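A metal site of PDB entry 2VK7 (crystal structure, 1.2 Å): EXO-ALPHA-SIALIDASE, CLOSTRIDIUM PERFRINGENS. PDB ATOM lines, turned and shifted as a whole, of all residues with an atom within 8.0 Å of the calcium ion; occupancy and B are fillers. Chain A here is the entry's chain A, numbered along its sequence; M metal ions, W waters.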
ATOM      1  N   ALA A  42       2.573  33.401  12.423  1.00  0.00           N
ATOM      2  CA  ALA A  42       2.591  32.633  13.665  1.00  0.00           C
ATOM      3  C   ALA A  42       2.829  31.180  13.272  1.00  0.00           C
ATOM      4  O   ALA A  42       1.900  30.496  12.789  1.00  0.00           O
ATOM      5  CB  ALA A  42       1.248  32.790  14.412  1.00  0.00           C
ATOM      6  N   ARG A  44       3.361  27.592  13.977  1.00  0.00           N
ATOM      7  CA  ARG A  44       2.885  26.875  15.176  1.00  0.00           C
ATOM      8  C   ARG A  44       3.698  25.667  15.559  1.00  0.00           C
ATOM      9  O   ARG A  44       3.601  25.195  16.692  1.00  0.00           O
ATOM     10  CB  ARG A  44       1.432  26.433  14.968  1.00  0.00           C
ATOM     11  CG  ARG A  44       0.458  27.546  14.737  1.00  0.00           C
ATOM     12  CD  ARG A  44       0.353  28.414  15.962  1.00  0.00           C
ATOM     13  NE  ARG A  44      -0.806  29.283  15.873  1.00  0.00           N
ATOM     14  CZ  ARG A  44      -1.338  29.931  16.901  1.00  0.00           C
ATOM     15  NH1 ARG A  44      -0.813  29.793  18.130  1.00  0.00           N
ATOM     16  NH2 ARG A  44      -2.391  30.704  16.708  1.00  0.00           N
ATOM     17  N   HIS A  45       4.457  25.124  14.607  1.00  0.00           N
ATOM     18  CA  HIS A  45       5.173  23.868  14.842  1.00  0.00           C
ATOM     19  C   HIS A  45       6.676  23.925  14.738  1.00  0.00           C
ATOM     20  O   HIS A  45       7.346  22.884  14.804  1.00  0.00           O
ATOM     21  CB  HIS A  45       4.593  22.766  13.960  1.00  0.00           C
ATOM     22  CG  HIS A  45       3.193  22.448  14.324  1.00  0.00           C
ATOM     23  ND1 HIS A  45       2.207  22.202  13.404  1.00  0.00           N
ATOM     24  CD2 HIS A  45       2.619  22.312  15.549  1.00  0.00           C
ATOM     25  CE1 HIS A  45       1.059  21.966  14.034  1.00  0.00           C
ATOM     26  NE2 HIS A  45       1.289  22.037  15.335  1.00  0.00           N
ATOM     27  N   ASN A  53       4.880  22.716   8.353  1.00  0.00           N
ATOM     28  CA  ASN A  53       4.416  23.553   9.461  1.00  0.00           C
ATOM     29  C   ASN A  53       2.917  23.721   9.369  1.00  0.00           C
ATOM     30  O   ASN A  53       2.272  23.181   8.435  1.00  0.00           O
ATOM     31  CB  ASN A  53       5.120  24.936   9.395  1.00  0.00           C
ATOM     32  CG  ASN A  53       5.448  25.486  10.783  1.00  0.00           C
ATOM     33  OD1 ASN A  53       4.647  25.337  11.705  1.00  0.00           O
ATOM     34  ND2 ASN A  53       6.585  26.145  10.907  1.00  0.00           N
ATOM     35  N   ASP A  54       2.408  24.501  10.302  1.00  0.00           N
ATOM     36  CA  ASP A  54       1.011  24.943  10.303  1.00  0.00           C
ATOM     37  C   ASP A  54       1.122  26.411  10.697  1.00  0.00           C
ATOM     38  O   ASP A  54       1.436  26.708  11.833  1.00  0.00           O
ATOM     39  CB  ASP A  54       0.174  24.109  11.279  1.00  0.00           C
ATOM     40  CG  ASP A  54      -1.319  24.314  11.090  1.00  0.00           C
ATOM     41  OD1 ASP A  54      -1.742  25.480  10.918  1.00  0.00           O
ATOM     42  OD2 ASP A  54      -2.111  23.336  11.220  1.00  0.00           O
ATOM     43  N   ILE A  55       0.887  27.318   9.745  1.00  0.00           N
ATOM     44  CA  ILE A  55       1.186  28.741   9.949  1.00  0.00           C
ATOM     45  C   ILE A  55      -0.090  29.541   9.816  1.00  0.00           C
ATOM     46  O   ILE A  55      -0.869  29.365   8.863  1.00  0.00           O
ATOM     47  CB  ILE A  55       2.218  29.219   8.908  1.00  0.00           C
ATOM     48  CG1 ILE A  55       3.444  28.289   8.910  1.00  0.00           C
ATOM     49  CG2 ILE A  55       2.566  30.688   9.216  1.00  0.00           C
ATOM     50  CD1 ILE A  55       4.459  28.590   7.785  1.00  0.00           C
ATOM     51  N   ASP A  56      -0.304  30.424  10.798  1.00  0.00           N
ATOM     52  CA  ASP A  56      -1.432  31.346  10.855  1.00  0.00           C
ATOM     53  C   ASP A  56      -0.909  32.774  10.724  1.00  0.00           C
ATOM     54  O   ASP A  56       0.301  33.018  10.918  1.00  0.00           O
ATOM     55  CB  ASP A  56      -2.106  31.187  12.218  1.00  0.00           C
ATOM     56  CG  ASP A  56      -2.509  29.744  12.521  1.00  0.00           C
ATOM     57  OD1 ASP A  56      -2.916  29.013  11.578  1.00  0.00           O
ATOM     58  OD2 ASP A  56      -2.460  29.396  13.737  1.00  0.00           O
ATOM     59  N   THR A  57      -1.779  33.703  10.390  1.00  0.00           N
ATOM     60  CA  THR A  57      -1.385  35.123  10.319  1.00  0.00           C
ATOM     61  C   THR A  57      -1.822  35.834  11.603  1.00  0.00           C
ATOM     62  O   THR A  57      -3.005  35.752  11.974  1.00  0.00           O
ATOM     63  CB  THR A  57      -2.068  35.834   9.122  1.00  0.00           C
ATOM     64  OG1 THR A  57      -1.653  35.185   7.906  1.00  0.00           O
ATOM     65  CG2 THR A  57      -1.690  37.305   9.112  1.00  0.00           C
ATOM     66  N   ILE A  74      -5.222  36.511  15.838  1.00  0.00           N
ATOM     67  CA  ILE A  74      -4.990  35.667  14.675  1.00  0.00           C
ATOM     68  C   ILE A  74      -6.098  35.958  13.693  1.00  0.00           C
ATOM     69  O   ILE A  74      -7.284  35.871  14.056  1.00  0.00           O
ATOM     70  CB  ILE A  74      -5.056  34.173  15.059  1.00  0.00           C
ATOM     71  CG1 ILE A  74      -3.977  33.804  16.085  1.00  0.00           C
ATOM     72  CG2 ILE A  74      -4.999  33.298  13.833  1.00  0.00           C
ATOM     73  CD1 ILE A  74      -2.590  33.995  15.613  1.00  0.00           C
ATOM     74  N   MET A  76      -6.093  34.761  10.186  1.00  0.00           N
ATOM     75  CA  MET A  76      -6.331  33.668   9.220  1.00  0.00           C
ATOM     76  C   MET A  76      -5.708  32.437   9.832  1.00  0.00           C
ATOM     77  O   MET A  76      -4.534  32.478  10.272  1.00  0.00           O
ATOM     78  CB  MET A  76      -5.711  33.939   7.822  1.00  0.00           C
ATOM     79  CG  MET A  76      -6.566  34.847   6.983  1.00  0.00           C
ATOM     80  SD  MET A  76      -5.813  35.288   5.401  1.00  0.00           S
ATOM     81  CE  MET A  76      -4.645  36.500   6.007  1.00  0.00           C
ATOM     82  N   ASP A  77      -6.464  31.320   9.852  1.00  0.00           N
ATOM     83  CA  ASP A  77      -6.002  30.063  10.458  1.00  0.00           C
ATOM     84  C   ASP A  77      -6.706  28.961   9.694  1.00  0.00           C
ATOM     85  O   ASP A  77      -7.921  28.806   9.804  1.00  0.00           O
ATOM     86  CB  ASP A  77      -6.391  30.031  11.950  1.00  0.00           C
ATOM     87  CG  ASP A  77      -6.117  28.697  12.652  1.00  0.00           C
ATOM     88  OD1 ASP A  77      -5.667  27.713  12.030  1.00  0.00           O
ATOM     89  OD2 ASP A  77      -6.438  28.609  13.894  1.00  0.00           O
ATOM     90  N   TYR A  78      -5.945  28.202   8.918  1.00  0.00           N
ATOM     91  CA  TYR A  78      -6.469  27.032   8.195  1.00  0.00           C
ATOM     92  C   TYR A  78      -6.069  25.762   8.969  1.00  0.00           C
ATOM     93  O   TYR A  78      -5.062  25.755   9.700  1.00  0.00           O
ATOM     94  CB  TYR A  78      -5.877  26.997   6.788  1.00  0.00           C
ATOM     95  CG  TYR A  78      -6.432  28.087   5.898  1.00  0.00           C
ATOM     96  CD1 TYR A  78      -5.873  29.366   5.878  1.00  0.00           C
ATOM     97  CD2 TYR A  78      -7.541  27.840   5.096  1.00  0.00           C
ATOM     98  CE1 TYR A  78      -6.376  30.340   5.066  1.00  0.00           C
ATOM     99  CE2 TYR A  78      -8.045  28.834   4.257  1.00  0.00           C
ATOM    100  CZ  TYR A  78      -7.449  30.077   4.235  1.00  0.00           C
ATOM    101  OH  TYR A  78      -7.874  31.068   3.419  1.00  0.00           O
ATOM    102  N   PRO A  79      -6.855  24.699   8.816  1.00  0.00           N
ATOM    103  CA  PRO A  79      -6.562  23.503   9.592  1.00  0.00           C
ATOM    104  C   PRO A  79      -5.501  22.622   9.005  1.00  0.00           C
ATOM    105  O   PRO A  79      -5.163  22.696   7.820  1.00  0.00           O
ATOM    106  CB  PRO A  79      -7.920  22.767   9.578  1.00  0.00           C
ATOM    107  CG  PRO A  79      -8.505  23.158   8.211  1.00  0.00           C
ATOM    108  CD  PRO A  79      -8.089  24.601   8.008  1.00  0.00           C
ATOM    109  N   ASP A  80      -4.986  21.734   9.866  1.00  0.00           N
ATOM    110  CA  ASP A  80      -4.317  20.539   9.389  1.00  0.00           C
ATOM    111  C   ASP A  80      -3.161  20.822   8.443  1.00  0.00           C
ATOM    112  O   ASP A  80      -3.036  20.176   7.412  1.00  0.00           O
ATOM    113  CB  ASP A  80      -5.328  19.556   8.783  1.00  0.00           C
ATOM    114  CG  ASP A  80      -4.731  18.158   8.502  1.00  0.00           C
ATOM    115  OD1 ASP A  80      -3.750  17.744   9.181  1.00  0.00           O
ATOM    116  OD2 ASP A  80      -5.279  17.500   7.604  1.00  0.00           O
ATOM    117  N   LYS A  81      -2.270  21.734   8.850  1.00  0.00           N
ATOM    118  CA  LYS A  81      -1.007  22.018   8.147  1.00  0.00           C
ATOM    119  C   LYS A  81      -1.243  22.680   6.787  1.00  0.00           C
ATOM    120  O   LYS A  81      -0.338  22.724   5.966  1.00  0.00           O
ATOM    121  CB  LYS A  81      -0.111  20.813   8.072  1.00  0.00           C
ATOM    122  CG  LYS A  81       0.303  20.249   9.429  1.00  0.00           C
ATOM    123  CD  LYS A  81       1.207  19.019   9.210  1.00  0.00           C
ATOM    124  CE  LYS A  81       2.637  19.418   8.761  1.00  0.00           C
ATOM    125  NZ  LYS A  81       3.442  18.215   8.563  1.00  0.00           N
ATOM    126  N   SER A  82      -2.447  23.214   6.586  1.00  0.00           N
ATOM    127  CA  SER A  82      -2.628  24.246   5.531  1.00  0.00           C
ATOM    128  C   SER A  82      -2.137  25.551   6.099  1.00  0.00           C
ATOM    129  O   SER A  82      -2.481  25.845   7.262  1.00  0.00           O
ATOM    130  CB  SER A  82      -4.082  24.317   5.148  1.00  0.00           C
ATOM    131  OG  SER A  82      -4.311  25.381   4.222  1.00  0.00           O
ATOM    132  N   SER A  83      -1.302  26.308   5.379  1.00  0.00           N
ATOM    133  CA  SER A  83      -0.624  27.474   5.935  1.00  0.00           C
ATOM    134  C   SER A  83      -0.900  28.745   5.122  1.00  0.00           C
ATOM    135  O   SER A  83      -1.064  28.690   3.887  1.00  0.00           O
ATOM    136  CB  SER A  83       0.903  27.276   5.933  1.00  0.00           C
ATOM    137  OG  SER A  83       1.260  26.384   6.968  1.00  0.00           O
ATOM    138  N   VAL A  84      -0.958  29.865   5.848  1.00  0.00           N
ATOM    139  CA  VAL A  84      -0.815  31.192   5.240  1.00  0.00           C
ATOM    140  C   VAL A  84       0.577  31.685   5.606  1.00  0.00           C
ATOM    141  O   VAL A  84       0.960  31.622   6.773  1.00  0.00           O
ATOM    142  CB  VAL A  84      -1.899  32.183   5.700  1.00  0.00           C
ATOM    143  CG1 VAL A  84      -3.152  32.009   4.865  1.00  0.00           C
ATOM    144  CG2 VAL A  84      -2.231  32.025   7.185  1.00  0.00           C
HETATM  145 CA    CA M   1      -3.656  26.746  11.309  1.00  0.00          CA
HETATM  146  O   HOH W   1      -3.062  26.827  13.676  1.00  0.00           O
HETATM  147  O   HOH W   2      -4.324  24.551  12.274  1.00  0.00           O
HETATM  148  O   HOH W   3      -3.091  27.786   9.157  1.00  0.00           O
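O of Asp 54 sits at hydrogen-bond distance from N of Arg 44 (3.0 Å). The side-chain carboxylate (OD2) of Asp 54 is in hydrogen-bond range of the backbone NH (N) of Lys 81 (2.9 Å). NE of Arg 44 lies within salt-bridge range of OD2 of Asp 56 (2.7 Å). O of Asp 56 is in hydrogen-bond range of N of Ala 42 (2.8 Å).
Within 4 Å of the calcium ion: Asp 54, Asp 56, Asp 77 and Tyr 78. The nearest printed residue that does not touch the calcium ion is Ser 82 (4.3 Å).
OD1 of Asp 54 is bound to the calcium ion (2.3 Å). The calcium ion is bound by OD1 of Asp 77, 2.3 Å away. The calcium ion is bound by O of Tyr 78 (2.4 Å). The side-chain carboxylate (OD1) of Asp 56 is bound to the calcium ion (2.4 Å). Water W1 binds the calcium ion (2.4 Å). Water W3 is bound to the calcium ion, 2.5 Å away. Water W2 binds the calcium ion (2.5 Å).
Water W3 lies within hydrogen-bond range of O of Ile 55, O of Ser 82 and N of Tyr 78.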
